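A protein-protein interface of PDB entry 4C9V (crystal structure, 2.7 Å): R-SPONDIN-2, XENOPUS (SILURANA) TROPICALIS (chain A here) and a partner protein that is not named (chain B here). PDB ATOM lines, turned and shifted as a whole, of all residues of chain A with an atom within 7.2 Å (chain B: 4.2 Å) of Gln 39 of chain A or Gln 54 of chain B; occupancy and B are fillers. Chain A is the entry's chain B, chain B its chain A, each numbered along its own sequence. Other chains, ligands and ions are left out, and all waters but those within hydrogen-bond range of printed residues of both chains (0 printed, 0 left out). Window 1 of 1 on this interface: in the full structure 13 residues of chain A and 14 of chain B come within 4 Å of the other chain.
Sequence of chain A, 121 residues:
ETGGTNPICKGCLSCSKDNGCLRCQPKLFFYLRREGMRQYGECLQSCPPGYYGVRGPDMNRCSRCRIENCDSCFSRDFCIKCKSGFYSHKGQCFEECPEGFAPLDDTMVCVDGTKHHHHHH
The backbone carbonyl oxygen (O) of Asp 18 of chain A sits at hydrogen-bond distance from the side-chain amide nitrogen (NE2) of Gln 54 of chain B.
The side-chain amide nitrogen of Gln 54 of chain B is in hydrogen-bond range of the side-chain amide oxygen of Asn 19 of chain A (3.5 Å).
NH2 of Arg 34 of chain A sits at hydrogen-bond distance from O of Gln 54 of chain B (2.6 Å).
The backbone carbonyl oxygen (O) of Met 37 of chain A is in hydrogen-bond range of the backbone NH (N) of Gln 54 of chain B, at 2.9 Å.
The side-chain amide nitrogen (NE2) of Gln 54 of chain B is in hydrogen-bond range of the backbone carbonyl oxygen (O) of Gln 39 of chain A (3.0 Å).
A ring nitrogen (NE2) of His 56 of chain B lies within hydrogen-bond range of the backbone carbonyl oxygen (O) of Asn 19 of chain A, at 2.8 Å.
N of His 56 of chain B lies within hydrogen-bond range of OE1 of Gln 39 of chain A, 3.1 Å away.
Printed residues of chain A that touch a printed residue of chain B: Asp 18, Asn 19, Leu 32, Arg 34, Gly 36, Met 37, Arg 38, Gln 39 and Gly 41.
Hydrophobic or aromatic side chains of chain A within 4 Å of the printed part of chain B: Leu 32 and Met 37.
Of the 7 printed residues of chain B, 6 touch a printed residue of chain A.
Hydrophobic or aromatic side chains of chain B that line the printed part of chain A: Leu 53, Phe 55, His 56 and Val 146.
Among the printed residues, no Asp or Glu carboxylate lies within 4 Å of a Lys or Arg side-chain nitrogen of the other chain.
Among the printed residues, pairs that only touch across the chains: Leu 32 of chain A with His 56 of chain B (3.4 Å), Leu 32 of chain A with Ser 59 of chain B (3.7 Å), Arg 34 of chain A with Leu 53 of chain B (3.6 Å), Arg 34 of chain A with Phe 55 of chain B (3.6 Å), Gly 36 of chain A with Leu 53 of chain B (3.6 Å), Met 37 of chain A with Leu 53 of chain B (3.95 Å), Met 37 of chain A with Val 146 of chain B (3.7 Å), Arg 38 of chain A with Gln 54 of chain B (3.6 Å), Arg 38 of chain A with Val 146 of chain B (3.6 Å), Gln 39 of chain A with Phe 55 of chain B (3.3 Å), Gln 39 of chain A with Ser 59 of chain B (3.8 Å) and Gly 41 of chain A with His 56 of chain B (3.4 Å).
O of Leu 53 of chain B is in hydrogen-bond range of N of Ile 76 of chain B (3.0 Å).
The side-chain amino group (NZ) of Lys 17 of chain A is in salt-bridge range of the side-chain carboxylate (OD1) of Asp 18 of chain A.
The backbone carbonyl oxygen (O) of Lys 17 of chain A lies within hydrogen-bond range of the guanidinium group (NH2) of Arg 38 of chain A (3.3 Å).
The backbone NH (N) of Gly 41 of chain A is in hydrogen-bond range of the backbone carbonyl oxygen (O) of Asn 19 of chain A.
NH2 of Arg 34 of chain A is in hydrogen-bond range of O of Met 37 of chain A (3.0 Å).
The backbone carbonyl oxygen of Arg 38 of chain A sits at hydrogen-bond distance from the guanidinium group of Arg 34 of chain A (3.3 Å).
Gly 20 of chain A touches none of the printed residues of chain B.
Of the printed residues of chain B, Arg 38 of chain A touches Gln 54 (3.6 Å) and Val 146 (3.6 Å).
Gln 39 of chain A touches just these residues of chain B: Gln 54, Phe 55, His 56 and Ser 59.
Of the printed residues of chain A, Leu 53 of chain B touches Arg 34 (3.6 Å), Gly 36 (3.6 Å) and Met 37 (3.95 Å).
Of the printed residues of chain A, Gln 54 of chain B touches Asp 18, Asn 19, Arg 34, Met 37, Arg 38 and Gln 39.
The nearest residue of chain A that does not touch Gln 54 of chain B is Tyr 40 of chain A (5.0 Å).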
ATOM      1  N   LYS A  17      -8.783  13.822  12.325  1.00  0.00           N
ATOM      2  CA  LYS A  17      -9.695  13.547  11.207  1.00  0.00           C
ATOM      3  C   LYS A  17     -10.187  14.833  10.532  1.00  0.00           C
ATOM      4  O   LYS A  17     -10.450  14.843   9.327  1.00  0.00           O
ATOM      5  CB  LYS A  17     -10.885  12.693  11.665  1.00  0.00           C
ATOM      6  CG  LYS A  17     -11.896  13.415  12.544  1.00  0.00           C
ATOM      7  CD  LYS A  17     -12.938  12.452  13.091  1.00  0.00           C
ATOM      8  CE  LYS A  17     -14.086  13.193  13.760  1.00  0.00           C
ATOM      9  NZ  LYS A  17     -14.830  14.073  12.813  1.00  0.00           N
ATOM     10  N   ASP A  18     -10.301  15.910  11.312  1.00  0.00           N
ATOM     11  CA  ASP A  18     -10.782  17.201  10.809  1.00  0.00           C
ATOM     12  C   ASP A  18      -9.690  17.989  10.084  1.00  0.00           C
ATOM     13  O   ASP A  18      -9.936  18.555   9.017  1.00  0.00           O
ATOM     14  CB  ASP A  18     -11.341  18.046  11.960  1.00  0.00           C
ATOM     15  CG  ASP A  18     -12.512  17.379  12.665  1.00  0.00           C
ATOM     16  OD1 ASP A  18     -13.209  16.555  12.032  1.00  0.00           O
ATOM     17  OD2 ASP A  18     -12.739  17.681  13.858  1.00  0.00           O
ATOM     18  N   ASN A  19      -8.495  18.031  10.670  1.00  0.00           N
ATOM     19  CA  ASN A  19      -7.364  18.767  10.092  1.00  0.00           C
ATOM     20  C   ASN A  19      -6.424  17.898   9.257  1.00  0.00           C
ATOM     21  O   ASN A  19      -5.496  18.415   8.638  1.00  0.00           O
ATOM     22  CB  ASN A  19      -6.553  19.450  11.200  1.00  0.00           C
ATOM     23  CG  ASN A  19      -7.330  20.538  11.914  1.00  0.00           C
ATOM     24  OD1 ASN A  19      -8.114  21.264  11.305  1.00  0.00           O
ATOM     25  ND2 ASN A  19      -7.101  20.666  13.215  1.00  0.00           N
ATOM     26  N   GLY A  20      -6.656  16.587   9.241  1.00  0.00           N
ATOM     27  CA  GLY A  20      -5.766  15.661   8.542  1.00  0.00           C
ATOM     28  C   GLY A  20      -4.438  15.554   9.267  1.00  0.00           C
ATOM     29  O   GLY A  20      -4.403  15.469  10.493  1.00  0.00           O
ATOM     30  N   LEU A  32      -1.023  21.567   2.369  1.00  0.00           N
ATOM     31  CA  LEU A  32      -2.440  21.781   2.651  1.00  0.00           C
ATOM     32  C   LEU A  32      -3.277  21.573   1.393  1.00  0.00           C
ATOM     33  O   LEU A  32      -3.254  22.401   0.482  1.00  0.00           O
ATOM     34  CB  LEU A  32      -2.664  23.195   3.187  1.00  0.00           C
ATOM     35  CG  LEU A  32      -1.938  23.563   4.483  1.00  0.00           C
ATOM     36  CD1 LEU A  32      -2.017  25.062   4.742  1.00  0.00           C
ATOM     37  CD2 LEU A  32      -2.510  22.781   5.656  1.00  0.00           C
ATOM     38  N   ARG A  33      -4.009  20.462   1.345  1.00  0.00           N
ATOM     39  CA  ARG A  33      -4.889  20.167   0.220  1.00  0.00           C
ATOM     40  C   ARG A  33      -6.261  20.790   0.450  1.00  0.00           C
ATOM     41  O   ARG A  33      -6.905  20.528   1.466  1.00  0.00           O
ATOM     42  CB  ARG A  33      -5.024  18.656   0.021  1.00  0.00           C
ATOM     43  CG  ARG A  33      -5.960  18.274  -1.117  1.00  0.00           C
ATOM     44  CD  ARG A  33      -5.666  16.884  -1.663  1.00  0.00           C
ATOM     45  NE  ARG A  33      -4.356  16.807  -2.310  1.00  0.00           N
ATOM     46  CZ  ARG A  33      -4.061  17.317  -3.505  1.00  0.00           C
ATOM     47  NH1 ARG A  33      -4.977  17.964  -4.225  1.00  0.00           N
ATOM     48  NH2 ARG A  33      -2.829  17.180  -3.988  1.00  0.00           N
ATOM     49  N   ARG A  34      -6.703  21.611  -0.500  1.00  0.00           N
ATOM     50  CA  ARG A  34      -8.014  22.250  -0.426  1.00  0.00           C
ATOM     51  C   ARG A  34      -9.068  21.358  -1.075  1.00  0.00           C
ATOM     52  O   ARG A  34      -8.761  20.569  -1.970  1.00  0.00           O
ATOM     53  CB  ARG A  34      -7.987  23.617  -1.120  1.00  0.00           C
ATOM     54  CG  ARG A  34      -9.110  24.551  -0.697  1.00  0.00           C
ATOM     55  CD  ARG A  34      -8.844  25.177   0.668  1.00  0.00           C
ATOM     56  NE  ARG A  34     -10.073  25.405   1.432  1.00  0.00           N
ATOM     57  CZ  ARG A  34     -10.158  26.145   2.536  1.00  0.00           C
ATOM     58  NH1 ARG A  34      -9.090  26.757   3.040  1.00  0.00           N
ATOM     59  NH2 ARG A  34     -11.329  26.276   3.148  1.00  0.00           N
ATOM     60  N   GLU A  35     -10.307  21.483  -0.610  1.00  0.00           N
ATOM     61  CA  GLU A  35     -11.422  20.730  -1.172  1.00  0.00           C
ATOM     62  C   GLU A  35     -12.736  21.478  -0.927  1.00  0.00           C
ATOM     63  O   GLU A  35     -13.590  21.035  -0.155  1.00  0.00           O
ATOM     64  CB  GLU A  35     -11.449  19.320  -0.573  1.00  0.00           C
ATOM     65  CG  GLU A  35     -12.381  18.349  -1.279  1.00  0.00           C
ATOM     66  CD  GLU A  35     -12.362  16.968  -0.653  1.00  0.00           C
ATOM     67  OE1 GLU A  35     -11.266  16.494  -0.280  1.00  0.00           O
ATOM     68  OE2 GLU A  35     -13.442  16.350  -0.535  1.00  0.00           O
ATOM     69  N   GLY A  36     -12.876  22.624  -1.589  1.00  0.00           N
ATOM     70  CA  GLY A  36     -14.075  23.454  -1.476  1.00  0.00           C
ATOM     71  C   GLY A  36     -14.167  24.141  -0.127  1.00  0.00           C
ATOM     72  O   GLY A  36     -13.628  25.233   0.062  1.00  0.00           O
ATOM     73  N   MET A  37     -14.861  23.495   0.806  1.00  0.00           N
ATOM     74  CA  MET A  37     -14.951  23.975   2.185  1.00  0.00           C
ATOM     75  C   MET A  37     -13.813  23.399   3.025  1.00  0.00           C
ATOM     76  O   MET A  37     -13.261  24.089   3.881  1.00  0.00           O
ATOM     77  CB  MET A  37     -16.300  23.590   2.803  1.00  0.00           C
ATOM     78  CG  MET A  37     -17.502  24.233   2.127  1.00  0.00           C
ATOM     79  SD  MET A  37     -19.052  23.979   3.019  1.00  0.00           S
ATOM     80  CE  MET A  37     -19.283  22.215   2.815  1.00  0.00           C
ATOM     81  N   ARG A  38     -13.468  22.138   2.771  1.00  0.00           N
ATOM     82  CA  ARG A  38     -12.463  21.427   3.561  1.00  0.00           C
ATOM     83  C   ARG A  38     -11.032  21.864   3.258  1.00  0.00           C
ATOM     84  O   ARG A  38     -10.710  22.233   2.128  1.00  0.00           O
ATOM     85  CB  ARG A  38     -12.564  19.918   3.324  1.00  0.00           C
ATOM     86  CG  ARG A  38     -13.812  19.265   3.891  1.00  0.00           C
ATOM     87  CD  ARG A  38     -13.608  17.767   4.059  1.00  0.00           C
ATOM     88  NE  ARG A  38     -12.616  17.468   5.092  1.00  0.00           N
ATOM     89  CZ  ARG A  38     -12.152  16.250   5.372  1.00  0.00           C
ATOM     90  NH1 ARG A  38     -12.584  15.186   4.699  1.00  0.00           N
ATOM     91  NH2 ARG A  38     -11.247  16.094   6.333  1.00  0.00           N
ATOM     92  N   GLN A  39     -10.185  21.813   4.285  1.00  0.00           N
ATOM     93  CA  GLN A  39      -8.737  21.962   4.131  1.00  0.00           C
ATOM     94  C   GLN A  39      -8.029  21.057   5.138  1.00  0.00           C
ATOM     95  O   GLN A  39      -8.117  21.277   6.346  1.00  0.00           O
ATOM     96  CB  GLN A  39      -8.296  23.412   4.337  1.00  0.00           C
ATOM     97  CG  GLN A  39      -6.829  23.646   4.005  1.00  0.00           C
ATOM     98  CD  GLN A  39      -6.404  25.092   4.173  1.00  0.00           C
ATOM     99  OE1 GLN A  39      -6.767  25.747   5.145  1.00  0.00           O
ATOM    100  NE2 GLN A  39      -5.619  25.591   3.228  1.00  0.00           N
ATOM    101  N   TYR A  40      -7.332  20.043   4.633  1.00  0.00           N
ATOM    102  CA  TYR A  40      -6.628  19.090   5.486  1.00  0.00           C
ATOM    103  C   TYR A  40      -5.182  18.920   5.035  1.00  0.00           C
ATOM    104  O   TYR A  40      -4.880  19.010   3.844  1.00  0.00           O
ATOM    105  CB  TYR A  40      -7.355  17.743   5.502  1.00  0.00           C
ATOM    106  CG  TYR A  40      -7.456  17.061   4.154  1.00  0.00           C
ATOM    107  CD1 TYR A  40      -8.465  17.398   3.254  1.00  0.00           C
ATOM    108  CD2 TYR A  40      -6.553  16.069   3.786  1.00  0.00           C
ATOM    109  CE1 TYR A  40      -8.563  16.774   2.021  1.00  0.00           C
ATOM    110  CE2 TYR A  40      -6.643  15.437   2.557  1.00  0.00           C
ATOM    111  CZ  TYR A  40      -7.648  15.791   1.677  1.00  0.00           C
ATOM    112  OH  TYR A  40      -7.738  15.163   0.455  1.00  0.00           O
ATOM    113  N   GLY A  41      -4.296  18.677   5.996  1.00  0.00           N
ATOM    114  CA  GLY A  41      -2.871  18.534   5.722  1.00  0.00           C
ATOM    115  C   GLY A  41      -2.512  17.173   5.156  1.00  0.00           C
ATOM    116  O   GLY A  41      -3.236  16.197   5.346  1.00  0.00           O
ATOM    117  N   LEU B  53     -15.632  28.414   5.410  1.00  0.00           N
ATOM    118  CA  LEU B  53     -14.371  27.873   4.912  1.00  0.00           C
ATOM    119  C   LEU B  53     -13.505  27.373   6.065  1.00  0.00           C
ATOM    120  O   LEU B  53     -13.176  28.137   6.975  1.00  0.00           O
ATOM    121  CB  LEU B  53     -13.614  28.944   4.126  1.00  0.00           C
ATOM    122  CG  LEU B  53     -14.270  29.430   2.830  1.00  0.00           C
ATOM    123  CD1 LEU B  53     -13.446  30.540   2.187  1.00  0.00           C
ATOM    124  CD2 LEU B  53     -14.472  28.275   1.856  1.00  0.00           C
ATOM    125  N   GLN B  54     -13.144  26.092   6.025  1.00  0.00           N
ATOM    126  CA  GLN B  54     -12.242  25.512   7.017  1.00  0.00           C
ATOM    127  C   GLN B  54     -10.823  26.000   6.762  1.00  0.00           C
ATOM    128  O   GLN B  54     -10.438  26.224   5.616  1.00  0.00           O
ATOM    129  CB  GLN B  54     -12.279  23.980   6.963  1.00  0.00           C
ATOM    130  CG  GLN B  54     -11.589  23.293   8.137  1.00  0.00           C
ATOM    131  CD  GLN B  54     -11.227  21.842   7.856  1.00  0.00           C
ATOM    132  OE1 GLN B  54     -11.880  21.161   7.063  1.00  0.00           O
ATOM    133  NE2 GLN B  54     -10.178  21.360   8.515  1.00  0.00           N
ATOM    134  N   PHE B  55     -10.055  26.178   7.833  1.00  0.00           N
ATOM    135  CA  PHE B  55      -8.644  26.527   7.709  1.00  0.00           C
ATOM    136  C   PHE B  55      -7.791  25.722   8.690  1.00  0.00           C
ATOM    137  O   PHE B  55      -8.146  25.568   9.858  1.00  0.00           O
ATOM    138  CB  PHE B  55      -8.436  28.029   7.914  1.00  0.00           C
ATOM    139  CG  PHE B  55      -8.933  28.870   6.772  1.00  0.00           C
ATOM    140  CD1 PHE B  55      -8.113  29.145   5.685  1.00  0.00           C
ATOM    141  CD2 PHE B  55     -10.223  29.387   6.783  1.00  0.00           C
ATOM    142  CE1 PHE B  55      -8.569  29.920   4.629  1.00  0.00           C
ATOM    143  CE2 PHE B  55     -10.684  30.164   5.731  1.00  0.00           C
ATOM    144  CZ  PHE B  55      -9.857  30.430   4.653  1.00  0.00           C
ATOM    145  N   HIS B  56      -6.671  25.207   8.191  1.00  0.00           N
ATOM    146  CA  HIS B  56      -5.724  24.446   8.999  1.00  0.00           C
ATOM    147  C   HIS B  56      -4.988  25.416   9.921  1.00  0.00           C
ATOM    148  O   HIS B  56      -4.656  26.521   9.502  1.00  0.00           O
ATOM    149  CB  HIS B  56      -4.719  23.740   8.086  1.00  0.00           C
ATOM    150  CG  HIS B  56      -4.171  22.465   8.644  1.00  0.00           C
ATOM    151  ND1 HIS B  56      -3.195  22.431   9.613  1.00  0.00           N
ATOM    152  CD2 HIS B  56      -4.446  21.175   8.342  1.00  0.00           C
ATOM    153  CE1 HIS B  56      -2.901  21.175   9.899  1.00  0.00           C
ATOM    154  NE2 HIS B  56      -3.647  20.392   9.140  1.00  0.00           N
ATOM    155  N   SER B  59      -2.073  26.882   8.357  1.00  0.00           N
ATOM    156  CA  SER B  59      -2.378  27.764   7.232  1.00  0.00           C
ATOM    157  C   SER B  59      -2.172  29.212   7.648  1.00  0.00           C
ATOM    158  O   SER B  59      -1.518  29.980   6.945  1.00  0.00           O
ATOM    159  CB  SER B  59      -3.818  27.567   6.753  1.00  0.00           C
ATOM    160  OG  SER B  59      -4.077  28.337   5.591  1.00  0.00           O
ATOM    161  N   ILE B  76     -13.485  28.735   9.869  1.00  0.00           N
ATOM    162  CA  ILE B  76     -13.656  27.763  10.951  1.00  0.00           C
ATOM    163  C   ILE B  76     -12.357  26.978  11.119  1.00  0.00           C
ATOM    164  O   ILE B  76     -11.955  26.221  10.238  1.00  0.00           O
ATOM    165  CB  ILE B  76     -14.883  26.830  10.731  1.00  0.00           C
ATOM    166  CG1 ILE B  76     -14.916  25.698  11.767  1.00  0.00           C
ATOM    167  CG2 ILE B  76     -14.911  26.231   9.333  1.00  0.00           C
ATOM    168  CD1 ILE B  76     -14.923  26.168  13.206  1.00  0.00           C
ATOM    169  N   VAL B 146     -19.329  20.706   7.076  1.00  0.00           N
ATOM    170  CA  VAL B 146     -18.151  20.946   6.239  1.00  0.00           C
ATOM    171  C   VAL B 146     -17.661  19.628   5.639  1.00  0.00           C
ATOM    172  O   VAL B 146     -17.307  19.570   4.460  1.00  0.00           O
ATOM    173  CB  VAL B 146     -17.008  21.614   7.039  1.00  0.00           C
ATOM    174  CG1 VAL B 146     -15.749  21.742   6.187  1.00  0.00           C
ATOM    175  CG2 VAL B 146     -17.442  22.978   7.557  1.00  0.00           C
